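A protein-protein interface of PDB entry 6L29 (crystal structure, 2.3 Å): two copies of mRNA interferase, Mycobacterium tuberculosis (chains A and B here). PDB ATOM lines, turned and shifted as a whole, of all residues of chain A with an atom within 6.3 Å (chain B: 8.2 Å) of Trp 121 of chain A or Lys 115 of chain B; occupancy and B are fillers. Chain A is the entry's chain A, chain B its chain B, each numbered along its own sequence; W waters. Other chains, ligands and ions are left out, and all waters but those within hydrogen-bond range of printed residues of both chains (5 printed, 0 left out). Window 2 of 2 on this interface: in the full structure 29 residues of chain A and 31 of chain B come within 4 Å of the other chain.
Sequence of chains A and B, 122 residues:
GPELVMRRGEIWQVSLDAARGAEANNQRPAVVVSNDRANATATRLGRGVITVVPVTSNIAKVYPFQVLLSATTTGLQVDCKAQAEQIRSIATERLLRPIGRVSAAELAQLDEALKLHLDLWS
CD2 of Leu 120 of chain B touches OD1 of Asp 111 of chain A, 3.7 Å away.
Lys 115 of chain A touches Leu 120 of chain B (CG to CD1, 3.9 Å).
Arg 8 of chain B touches Asp 119 of chain A.
Leu 120 of chain A touches Arg 8 of chain B.
Leu 120 of chain A touches Asp 111 of chain B.
Leu 114 of chain B touches Leu 120 of chain A (CB to CD1, 3.9 Å).
Leu 120 of chain B touches Leu 120 of chain A.
Trp 121 of chain A touches Lys 115 of chain B.
Of the printed residues of chain B, Lys 115 of chain A touches Leu 120.
Of the printed residues of chain B, Leu 116 of chain A touches Asn 35 (3.4 Å).
Printed residues of chain B within 4 Å of Asp 119 of chain A: Arg 8 (3.8 Å).
Of the printed residues of chain A, Leu 114 of chain B touches Leu 120.
Lys 115 of chain B touches just one residue of chain A: Trp 121 (3.7 Å).
Asp 111 of chain A touches Leu 120 of chain B, and with the chains exchanged Leu 120 of chain A touches Asp 111 of chain B.
Lys 115 of chain A touches Leu 120 of chain B, but with the chains exchanged Leu 120 of chain A does not touch Lys 115 of chain B (4.3 Å).
Leu 120 of chain B touches its own counterpart, Leu 120 of chain A.
Trp 121 of chain A touches Lys 115 of chain B, but with the chains exchanged Lys 115 of chain A does not touch Trp 121 of chain B (4.4 Å).
9 positions are printed for both chains.
Of the 10 pairs that touch across the chains among the printed residues, 3 have their exchanged pair printed and touching as well.
Of the 20 printed residues of chain B, 6 touch a printed residue of chain A.
Printed residues of chain B that touch a printed residue of chain A: Arg 8, Asn 35, Asp 111, Leu 114, Lys 115 and Leu 120.
Hydrophobic or aromatic side chains of chain B within 4 Å of the printed part of chain A: Leu 114 and Leu 120.
Hydrophobic or aromatic side chains of chain A that line the printed part of chain B: Leu 120.
Among the printed residues, 10 pairs touch across the chains.
Water W3 lies within hydrogen-bond range of the side-chain carboxylate of Asp 111 of chain A (2.5 Å) and the backbone carbonyl oxygen of Asp 119 of chain B (2.8 Å).
Water W4 bridges OD2 of Asp 111 of chain B (2.6 Å) and O of Asp 119 of chain A (2.9 Å).
Water W5 lies within hydrogen-bond range of the backbone carbonyl oxygen of Leu 116 of chain A, the side-chain carboxylate of Asp 119 of chain A and the guanidinium group of Arg 37 of chain B.
Water W1 bridges NZ of Lys 115 of chain B (2.7 Å) and O of Trp 121 of chain A (3.3 Å).
Water W2 lies within hydrogen-bond range of NZ of Lys 115 of chain A (3.1 Å) and N of Trp 121 of chain B (3.4 Å).
OE1 of Glu 112 of chain A is in salt-bridge range of NZ of Lys 115 of chain A (3.1 Å).
The backbone carbonyl oxygen of Lys 115 of chain A is in hydrogen-bond range of the backbone NH of Leu 120 of chain A (2.9 Å).
The indole nitrogen (NE1) of Trp 121 of chain A is in hydrogen-bond range of the backbone carbonyl oxygen (O) of Lys 115 of chain A (3.3 Å).
The guanidinium group (NH2) of Arg 8 of chain B is in salt-bridge range of the side-chain carboxylate (OD1) of Asp 111 of chain B, 2.8 Å away.
The side-chain amide oxygen of Asn 35 of chain B lies within hydrogen-bond range of the backbone NH of Arg 37 of chain B.
The side-chain amino group (NZ) of Lys 115 of chain B is in salt-bridge range of the side-chain carboxylate (OE1) of Glu 112 of chain B.
The backbone carbonyl oxygen (O) of Leu 116 of chain A is in hydrogen-bond range of the side-chain amide nitrogen (ND2) of Asn 35 of chain B (3.4 Å).
The backbone NH of Asn 35 of chain B is in hydrogen-bond range of the backbone carbonyl oxygen of His 117 of chain A (2.9 Å).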
ATOM      1  N   ASP A 111      -7.878  22.332 -22.985  1.00  0.00           N
ATOM      2  CA  ASP A 111      -8.412  21.259 -23.819  1.00  0.00           C
ATOM      3  C   ASP A 111      -9.250  20.296 -22.990  1.00  0.00           C
ATOM      4  O   ASP A 111     -10.357  19.915 -23.390  1.00  0.00           O
ATOM      5  CB  ASP A 111      -7.274  20.506 -24.505  1.00  0.00           C
ATOM      6  CG  ASP A 111      -6.491  21.375 -25.452  1.00  0.00           C
ATOM      7  OD1 ASP A 111      -6.986  22.469 -25.793  1.00  0.00           O
ATOM      8  OD2 ASP A 111      -5.384  20.964 -25.856  1.00  0.00           O
ATOM      9  N   GLU A 112      -8.729  19.877 -21.831  1.00  0.00           N
ATOM     10  CA  GLU A 112      -9.516  19.015 -20.952  1.00  0.00           C
ATOM     11  C   GLU A 112     -10.839  19.674 -20.579  1.00  0.00           C
ATOM     12  O   GLU A 112     -11.891  19.022 -20.576  1.00  0.00           O
ATOM     13  CB  GLU A 112      -8.719  18.677 -19.690  1.00  0.00           C
ATOM     14  CG  GLU A 112      -7.476  17.820 -19.927  1.00  0.00           C
ATOM     15  CD  GLU A 112      -7.770  16.556 -20.713  1.00  0.00           C
ATOM     16  OE1 GLU A 112      -7.323  16.455 -21.875  1.00  0.00           O
ATOM     17  OE2 GLU A 112      -8.455  15.663 -20.172  1.00  0.00           O
ATOM     18  N   ALA A 113     -10.805  20.971 -20.266  1.00  0.00           N
ATOM     19  CA  ALA A 113     -12.016  21.678 -19.875  1.00  0.00           C
ATOM     20  C   ALA A 113     -13.018  21.730 -21.023  1.00  0.00           C
ATOM     21  O   ALA A 113     -14.225  21.583 -20.806  1.00  0.00           O
ATOM     22  CB  ALA A 113     -11.657  23.085 -19.393  1.00  0.00           C
ATOM     23  N   LYS A 115     -13.236  19.514 -23.517  1.00  0.00           N
ATOM     24  CA  LYS A 115     -13.765  18.165 -23.683  1.00  0.00           C
ATOM     25  C   LYS A 115     -14.801  17.835 -22.615  1.00  0.00           C
ATOM     26  O   LYS A 115     -15.797  17.153 -22.895  1.00  0.00           O
ATOM     27  CB  LYS A 115     -12.626  17.149 -23.649  1.00  0.00           C
ATOM     28  CG  LYS A 115     -11.655  17.268 -24.809  1.00  0.00           C
ATOM     29  CD  LYS A 115     -10.728  16.068 -24.849  1.00  0.00           C
ATOM     30  CE  LYS A 115      -9.280  16.475 -24.685  1.00  0.00           C
ATOM     31  NZ  LYS A 115      -8.399  15.283 -24.531  1.00  0.00           N
ATOM     32  N   LEU A 116     -14.577  18.292 -21.383  1.00  0.00           N
ATOM     33  CA  LEU A 116     -15.562  18.080 -20.329  1.00  0.00           C
ATOM     34  C   LEU A 116     -16.843  18.856 -20.617  1.00  0.00           C
ATOM     35  O   LEU A 116     -17.947  18.303 -20.542  1.00  0.00           O
ATOM     36  CB  LEU A 116     -14.974  18.489 -18.978  1.00  0.00           C
ATOM     37  CG  LEU A 116     -15.887  18.322 -17.767  1.00  0.00           C
ATOM     38  CD1 LEU A 116     -16.151  16.846 -17.509  1.00  0.00           C
ATOM     39  CD2 LEU A 116     -15.282  18.976 -16.553  1.00  0.00           C
ATOM     40  N   HIS A 117     -16.709  20.140 -20.965  1.00  0.00           N
ATOM     41  CA  HIS A 117     -17.886  20.977 -21.161  1.00  0.00           C
ATOM     42  C   HIS A 117     -18.713  20.515 -22.354  1.00  0.00           C
ATOM     43  O   HIS A 117     -19.948  20.504 -22.291  1.00  0.00           O
ATOM     44  CB  HIS A 117     -17.489  22.440 -21.349  1.00  0.00           C
ATOM     45  CG  HIS A 117     -18.649  23.318 -21.696  1.00  0.00           C
ATOM     46  ND1 HIS A 117     -19.659  23.597 -20.802  1.00  0.00           N
ATOM     47  CD2 HIS A 117     -18.994  23.926 -22.855  1.00  0.00           C
ATOM     48  CE1 HIS A 117     -20.563  24.364 -21.386  1.00  0.00           C
ATOM     49  NE2 HIS A 117     -20.183  24.575 -22.634  1.00  0.00           N
ATOM     50  N   ASP A 119     -18.535  17.481 -23.770  1.00  0.00           N
ATOM     51  CA  ASP A 119     -18.735  16.030 -23.749  1.00  0.00           C
ATOM     52  C   ASP A 119     -18.086  15.374 -24.971  1.00  0.00           C
ATOM     53  O   ASP A 119     -18.717  14.609 -25.706  1.00  0.00           O
ATOM     54  CB  ASP A 119     -20.226  15.679 -23.651  1.00  0.00           C
ATOM     55  CG  ASP A 119     -20.464  14.269 -23.169  1.00  0.00           C
ATOM     56  OD1 ASP A 119     -21.573  13.750 -23.405  1.00  0.00           O
ATOM     57  OD2 ASP A 119     -19.542  13.680 -22.561  1.00  0.00           O
ATOM     58  N   LEU A 120     -16.802  15.678 -25.174  1.00  0.00           N
ATOM     59  CA  LEU A 120     -16.009  15.184 -26.298  1.00  0.00           C
ATOM     60  C   LEU A 120     -14.867  14.345 -25.731  1.00  0.00           C
ATOM     61  O   LEU A 120     -13.766  14.854 -25.510  1.00  0.00           O
ATOM     62  CB  LEU A 120     -15.471  16.336 -27.129  1.00  0.00           C
ATOM     63  CG  LEU A 120     -16.436  17.419 -27.616  1.00  0.00           C
ATOM     64  CD1 LEU A 120     -15.650  18.542 -28.274  1.00  0.00           C
ATOM     65  CD2 LEU A 120     -17.481  16.837 -28.566  1.00  0.00           C
ATOM     66  N   TRP A 121     -15.121  13.056 -25.512  1.00  0.00           N
ATOM     67  CA  TRP A 121     -14.118  12.177 -24.913  1.00  0.00           C
ATOM     68  C   TRP A 121     -13.857  10.915 -25.735  1.00  0.00           C
ATOM     69  O   TRP A 121     -14.254  10.817 -26.899  1.00  0.00           O
ATOM     70  CB  TRP A 121     -14.535  11.783 -23.494  1.00  0.00           C
ATOM     71  CG  TRP A 121     -14.405  12.893 -22.495  1.00  0.00           C
ATOM     72  CD1 TRP A 121     -15.416  13.605 -21.915  1.00  0.00           C
ATOM     73  CD2 TRP A 121     -13.184  13.448 -21.996  1.00  0.00           C
ATOM     74  NE1 TRP A 121     -14.898  14.559 -21.067  1.00  0.00           N
ATOM     75  CE2 TRP A 121     -13.530  14.483 -21.102  1.00  0.00           C
ATOM     76  CE3 TRP A 121     -11.830  13.167 -22.216  1.00  0.00           C
ATOM     77  CZ2 TRP A 121     -12.577  15.235 -20.430  1.00  0.00           C
ATOM     78  CZ3 TRP A 121     -10.881  13.917 -21.544  1.00  0.00           C
ATOM     79  CH2 TRP A 121     -11.263  14.939 -20.662  1.00  0.00           C
ATOM     80  N   ARG B   8     -28.587  17.672 -24.842  1.00  0.00           N
ATOM     81  CA  ARG B   8     -27.600  17.562 -25.911  1.00  0.00           C
ATOM     82  C   ARG B   8     -28.166  16.809 -27.108  1.00  0.00           C
ATOM     83  O   ARG B   8     -28.826  15.777 -26.962  1.00  0.00           O
ATOM     84  CB  ARG B   8     -26.340  16.859 -25.404  1.00  0.00           C
ATOM     85  CG  ARG B   8     -25.078  17.217 -26.188  1.00  0.00           C
ATOM     86  CD  ARG B   8     -23.830  16.587 -25.597  1.00  0.00           C
ATOM     87  NE  ARG B   8     -22.637  17.064 -26.285  1.00  0.00           N
ATOM     88  CZ  ARG B   8     -22.140  16.528 -27.398  1.00  0.00           C
ATOM     89  NH1 ARG B   8     -22.723  15.477 -27.955  1.00  0.00           N
ATOM     90  NH2 ARG B   8     -21.052  17.045 -27.953  1.00  0.00           N
ATOM     91  N   ASN B  35     -22.703  19.696 -22.334  1.00  0.00           N
ATOM     92  CA  ASN B  35     -23.025  18.432 -21.689  1.00  0.00           C
ATOM     93  C   ASN B  35     -24.322  18.554 -20.890  1.00  0.00           C
ATOM     94  O   ASN B  35     -24.729  19.637 -20.471  1.00  0.00           O
ATOM     95  CB  ASN B  35     -21.891  17.969 -20.769  1.00  0.00           C
ATOM     96  CG  ASN B  35     -21.792  18.800 -19.505  1.00  0.00           C
ATOM     97  OD1 ASN B  35     -22.505  18.564 -18.529  1.00  0.00           O
ATOM     98  ND2 ASN B  35     -20.890  19.774 -19.514  1.00  0.00           N
ATOM     99  N   ARG B  37     -25.220  17.818 -17.967  1.00  0.00           N
ATOM    100  CA  ARG B  37     -25.236  18.113 -16.539  1.00  0.00           C
ATOM    101  C   ARG B  37     -25.267  19.623 -16.357  1.00  0.00           C
ATOM    102  O   ARG B  37     -25.995  20.166 -15.513  1.00  0.00           O
ATOM    103  CB  ARG B  37     -24.045  17.445 -15.885  1.00  0.00           C
ATOM    104  CG  ARG B  37     -24.270  15.928 -15.783  1.00  0.00           C
ATOM    105  CD  ARG B  37     -23.017  15.113 -15.475  1.00  0.00           C
ATOM    106  NE  ARG B  37     -22.126  15.072 -16.635  1.00  0.00           N
ATOM    107  CZ  ARG B  37     -21.057  15.847 -16.769  1.00  0.00           C
ATOM    108  NH1 ARG B  37     -20.763  16.700 -15.803  1.00  0.00           N
ATOM    109  NH2 ARG B  37     -20.293  15.776 -17.857  1.00  0.00           N
ATOM    110  N   PRO B  64     -15.166  19.926 -43.592  1.00  0.00           N
ATOM    111  CA  PRO B  64     -15.039  18.820 -42.627  1.00  0.00           C
ATOM    112  C   PRO B  64     -15.473  19.190 -41.218  1.00  0.00           C
ATOM    113  O   PRO B  64     -15.827  18.293 -40.443  1.00  0.00           O
ATOM    114  CB  PRO B  64     -13.546  18.473 -42.684  1.00  0.00           C
ATOM    115  CG  PRO B  64     -12.887  19.715 -43.183  1.00  0.00           C
ATOM    116  CD  PRO B  64     -13.858  20.292 -44.167  1.00  0.00           C
ATOM    117  N   PHE B  65     -15.455  20.474 -40.856  1.00  0.00           N
ATOM    118  CA  PHE B  65     -15.960  20.924 -39.566  1.00  0.00           C
ATOM    119  C   PHE B  65     -17.447  21.270 -39.608  1.00  0.00           C
ATOM    120  O   PHE B  65     -17.947  21.936 -38.694  1.00  0.00           O
ATOM    121  CB  PHE B  65     -15.152  22.125 -39.064  1.00  0.00           C
ATOM    122  CG  PHE B  65     -14.875  23.158 -40.123  1.00  0.00           C
ATOM    123  CD1 PHE B  65     -15.809  24.139 -40.421  1.00  0.00           C
ATOM    124  CD2 PHE B  65     -13.676  23.149 -40.820  1.00  0.00           C
ATOM    125  CE1 PHE B  65     -15.553  25.086 -41.392  1.00  0.00           C
ATOM    126  CE2 PHE B  65     -13.415  24.094 -41.793  1.00  0.00           C
ATOM    127  CZ  PHE B  65     -14.353  25.064 -42.078  1.00  0.00           C
ATOM    128  N   ALA B  84     -19.683  23.790 -36.909  1.00  0.00           N
ATOM    129  CA  ALA B  84     -18.907  23.740 -35.670  1.00  0.00           C
ATOM    130  C   ALA B  84     -18.112  25.018 -35.456  1.00  0.00           C
ATOM    131  O   ALA B  84     -17.954  25.467 -34.316  1.00  0.00           O
ATOM    132  CB  ALA B  84     -17.965  22.534 -35.666  1.00  0.00           C
ATOM    133  N   ALA B 108     -22.682  12.148 -33.353  1.00  0.00           N
ATOM    134  CA  ALA B 108     -21.299  11.675 -33.334  1.00  0.00           C
ATOM    135  C   ALA B 108     -20.456  12.369 -34.401  1.00  0.00           C
ATOM    136  O   ALA B 108     -19.285  12.702 -34.163  1.00  0.00           O
ATOM    137  CB  ALA B 108     -21.263  10.160 -33.525  1.00  0.00           C
ATOM    138  N   GLN B 109     -21.038  12.592 -35.588  1.00  0.00           N
ATOM    139  CA  GLN B 109     -20.350  13.354 -36.626  1.00  0.00           C
ATOM    140  C   GLN B 109     -20.052  14.773 -36.161  1.00  0.00           C
ATOM    141  O   GLN B 109     -18.960  15.301 -36.405  1.00  0.00           O
ATOM    142  CB  GLN B 109     -21.192  13.388 -37.900  1.00  0.00           C
ATOM    143  CG  GLN B 109     -21.343  12.054 -38.599  1.00  0.00           C
ATOM    144  CD  GLN B 109     -22.470  12.072 -39.624  1.00  0.00           C
ATOM    145  OE1 GLN B 109     -23.107  11.053 -39.888  1.00  0.00           O
ATOM    146  NE2 GLN B 109     -22.716  13.233 -40.205  1.00  0.00           N
ATOM    147  N   LEU B 110     -21.021  15.408 -35.495  1.00  0.00           N
ATOM    148  CA  LEU B 110     -20.806  16.739 -34.940  1.00  0.00           C
ATOM    149  C   LEU B 110     -19.723  16.731 -33.870  1.00  0.00           C
ATOM    150  O   LEU B 110     -18.982  17.706 -33.739  1.00  0.00           O
ATOM    151  CB  LEU B 110     -22.117  17.286 -34.364  1.00  0.00           C
ATOM    152  CG  LEU B 110     -22.116  18.766 -33.958  1.00  0.00           C
ATOM    153  CD1 LEU B 110     -21.617  19.641 -35.101  1.00  0.00           C
ATOM    154  CD2 LEU B 110     -23.508  19.206 -33.515  1.00  0.00           C
ATOM    155  N   ASP B 111     -19.619  15.649 -33.093  1.00  0.00           N
ATOM    156  CA  ASP B 111     -18.538  15.546 -32.120  1.00  0.00           C
ATOM    157  C   ASP B 111     -17.188  15.501 -32.817  1.00  0.00           C
ATOM    158  O   ASP B 111     -16.234  16.161 -32.383  1.00  0.00           O
ATOM    159  CB  ASP B 111     -18.730  14.311 -31.242  1.00  0.00           C
ATOM    160  CG  ASP B 111     -19.976  14.398 -30.377  1.00  0.00           C
ATOM    161  OD1 ASP B 111     -20.536  15.503 -30.240  1.00  0.00           O
ATOM    162  OD2 ASP B 111     -20.395  13.358 -29.833  1.00  0.00           O
ATOM    163  N   GLU B 112     -17.087  14.738 -33.909  1.00  0.00           N
ATOM    164  CA  GLU B 112     -15.841  14.734 -34.669  1.00  0.00           C
ATOM    165  C   GLU B 112     -15.540  16.112 -35.240  1.00  0.00           C
ATOM    166  O   GLU B 112     -14.387  16.560 -35.225  1.00  0.00           O
ATOM    167  CB  GLU B 112     -15.902  13.693 -35.784  1.00  0.00           C
ATOM    168  CG  GLU B 112     -15.944  12.264 -35.272  1.00  0.00           C
ATOM    169  CD  GLU B 112     -14.868  11.985 -34.244  1.00  0.00           C
ATOM    170  OE1 GLU B 112     -15.227  11.671 -33.089  1.00  0.00           O
ATOM    171  OE2 GLU B 112     -13.664  12.080 -34.581  1.00  0.00           O
ATOM    172  N   ALA B 113     -16.567  16.807 -35.735  1.00  0.00           N
ATOM    173  CA  ALA B 113     -16.346  18.128 -36.315  1.00  0.00           C
ATOM    174  C   ALA B 113     -15.898  19.127 -35.253  1.00  0.00           C
ATOM    175  O   ALA B 113     -15.041  19.980 -35.517  1.00  0.00           O
ATOM    176  CB  ALA B 113     -17.612  18.608 -37.021  1.00  0.00           C
ATOM    177  N   LEU B 114     -16.461  19.028 -34.043  1.00  0.00           N
ATOM    178  CA  LEU B 114     -16.025  19.871 -32.933  1.00  0.00           C
ATOM    179  C   LEU B 114     -14.591  19.551 -32.526  1.00  0.00           C
ATOM    180  O   LEU B 114     -13.810  20.462 -32.228  1.00  0.00           O
ATOM    181  CB  LEU B 114     -16.969  19.709 -31.740  1.00  0.00           C
ATOM    182  CG  LEU B 114     -18.367  20.327 -31.886  1.00  0.00           C
ATOM    183  CD1 LEU B 114     -19.293  19.931 -30.736  1.00  0.00           C
ATOM    184  CD2 LEU B 114     -18.268  21.838 -31.986  1.00  0.00           C
ATOM    185  N   LYS B 115     -14.229  18.265 -32.502  1.00  0.00           N
ATOM    186  CA  LYS B 115     -12.847  17.892 -32.207  1.00  0.00           C
ATOM    187  C   LYS B 115     -11.889  18.478 -33.238  1.00  0.00           C
ATOM    188  O   LYS B 115     -10.828  19.007 -32.886  1.00  0.00           O
ATOM    189  CB  LYS B 115     -12.705  16.370 -32.157  1.00  0.00           C
ATOM    190  CG  LYS B 115     -13.285  15.701 -30.921  1.00  0.00           C
ATOM    191  CD  LYS B 115     -13.277  14.191 -31.092  1.00  0.00           C
ATOM    192  CE  LYS B 115     -13.989  13.494 -29.948  1.00  0.00           C
ATOM    193  NZ  LYS B 115     -14.449  12.121 -30.316  1.00  0.00           N
ATOM    194  N   LEU B 116     -12.251  18.396 -34.521  1.00  0.00           N
ATOM    195  CA  LEU B 116     -11.407  18.957 -35.574  1.00  0.00           C
ATOM    196  C   LEU B 116     -11.269  20.466 -35.421  1.00  0.00           C
ATOM    197  O   LEU B 116     -10.158  21.008 -35.455  1.00  0.00           O
ATOM    198  CB  LEU B 116     -11.991  18.615 -36.948  1.00  0.00           C
ATOM    199  CG  LEU B 116     -11.138  18.576 -38.224  1.00  0.00           C
ATOM    200  CD1 LEU B 116     -12.055  18.404 -39.420  1.00  0.00           C
ATOM    201  CD2 LEU B 116     -10.261  19.797 -38.426  1.00  0.00           C
ATOM    202  N   HIS B 117     -12.392  21.166 -35.261  1.00  0.00           N
ATOM    203  CA  HIS B 117     -12.349  22.623 -35.252  1.00  0.00           C
ATOM    204  C   HIS B 117     -11.553  23.158 -34.067  1.00  0.00           C
ATOM    205  O   HIS B 117     -10.812  24.141 -34.200  1.00  0.00           O
ATOM    206  CB  HIS B 117     -13.764  23.193 -35.237  1.00  0.00           C
ATOM    207  CG  HIS B 117     -13.800  24.686 -35.146  1.00  0.00           C
ATOM    208  ND1 HIS B 117     -13.259  25.502 -36.117  1.00  0.00           N
ATOM    209  CD2 HIS B 117     -14.292  25.511 -34.192  1.00  0.00           C
ATOM    210  CE1 HIS B 117     -13.422  26.765 -35.767  1.00  0.00           C
ATOM    211  NE2 HIS B 117     -14.048  26.797 -34.604  1.00  0.00           N
ATOM    212  N   LEU B 118     -11.690  22.525 -32.900  1.00  0.00           N
ATOM    213  CA  LEU B 118     -11.079  23.009 -31.667  1.00  0.00           C
ATOM    214  C   LEU B 118      -9.736  22.354 -31.367  1.00  0.00           C
ATOM    215  O   LEU B 118      -9.170  22.600 -30.296  1.00  0.00           O
ATOM    216  CB  LEU B 118     -12.037  22.804 -30.490  1.00  0.00           C
ATOM    217  CG  LEU B 118     -13.392  23.496 -30.650  1.00  0.00           C
ATOM    218  CD1 LEU B 118     -14.383  23.036 -29.589  1.00  0.00           C
ATOM    219  CD2 LEU B 118     -13.220  24.997 -30.601  1.00  0.00           C
ATOM    220  N   ASP B 119      -9.219  21.525 -32.281  1.00  0.00           N
ATOM    221  CA  ASP B 119      -7.894  20.914 -32.133  1.00  0.00           C
ATOM    222  C   ASP B 119      -7.834  19.994 -30.910  1.00  0.00           C
ATOM    223  O   ASP B 119      -6.823  19.926 -30.211  1.00  0.00           O
ATOM    224  CB  ASP B 119      -6.807  21.995 -32.066  1.00  0.00           C
ATOM    225  CG  ASP B 119      -5.533  21.606 -32.796  1.00  0.00           C
ATOM    226  OD1 ASP B 119      -5.599  20.789 -33.739  1.00  0.00           O
ATOM    227  OD2 ASP B 119      -4.459  22.137 -32.431  1.00  0.00           O
ATOM    228  N   LEU B 120      -8.924  19.270 -30.648  1.00  0.00           N
ATOM    229  CA  LEU B 120      -9.031  18.370 -29.501  1.00  0.00           C
ATOM    230  C   LEU B 120      -8.901  16.930 -29.987  1.00  0.00           C
ATOM    231  O   LEU B 120      -9.796  16.418 -30.664  1.00  0.00           O
ATOM    232  CB  LEU B 120     -10.359  18.569 -28.774  1.00  0.00           C
ATOM    233  CG  LEU B 120     -10.729  19.962 -28.276  1.00  0.00           C
ATOM    234  CD1 LEU B 120     -12.091  19.929 -27.610  1.00  0.00           C
ATOM    235  CD2 LEU B 120      -9.677  20.487 -27.313  1.00  0.00           C
ATOM    236  N   TRP B 121      -7.807  16.269 -29.624  1.00  0.00           N
ATOM    237  CA  TRP B 121      -7.542  14.917 -30.121  1.00  0.00           C
ATOM    238  C   TRP B 121      -7.536  13.872 -29.008  1.00  0.00           C
ATOM    239  O   TRP B 121      -6.570  13.763 -28.256  1.00  0.00           O
ATOM    240  CB  TRP B 121      -6.208  14.882 -30.873  1.00  0.00           C
ATOM    241  CG  TRP B 121      -6.104  15.940 -31.933  1.00  0.00           C
ATOM    242  CD1 TRP B 121      -5.760  17.251 -31.756  1.00  0.00           C
ATOM    243  CD2 TRP B 121      -6.361  15.779 -33.335  1.00  0.00           C
ATOM    244  NE1 TRP B 121      -5.781  17.915 -32.961  1.00  0.00           N
ATOM    245  CE2 TRP B 121      -6.148  17.034 -33.945  1.00  0.00           C
ATOM    246  CE3 TRP B 121      -6.748  14.697 -34.133  1.00  0.00           C
ATOM    247  CZ2 TRP B 121      -6.308  17.234 -35.318  1.00  0.00           C
ATOM    248  CZ3 TRP B 121      -6.903  14.897 -35.496  1.00  0.00           C
ATOM    249  CH2 TRP B 121      -6.684  16.156 -36.073  1.00  0.00           C
HETATM  250  O   HOH W   1     -16.660  12.173 -28.725  1.00  0.00           O
HETATM  251  O   HOH W   2      -6.637  16.915 -26.481  1.00  0.00           O
HETATM  252  O   HOH W   3      -4.832  20.495 -28.288  1.00  0.00           O
HETATM  253  O   HOH W   4     -20.400  12.880 -27.326  1.00  0.00           O
HETATM  254  O   HOH W   5     -18.338  15.643 -20.401  1.00  0.00           O
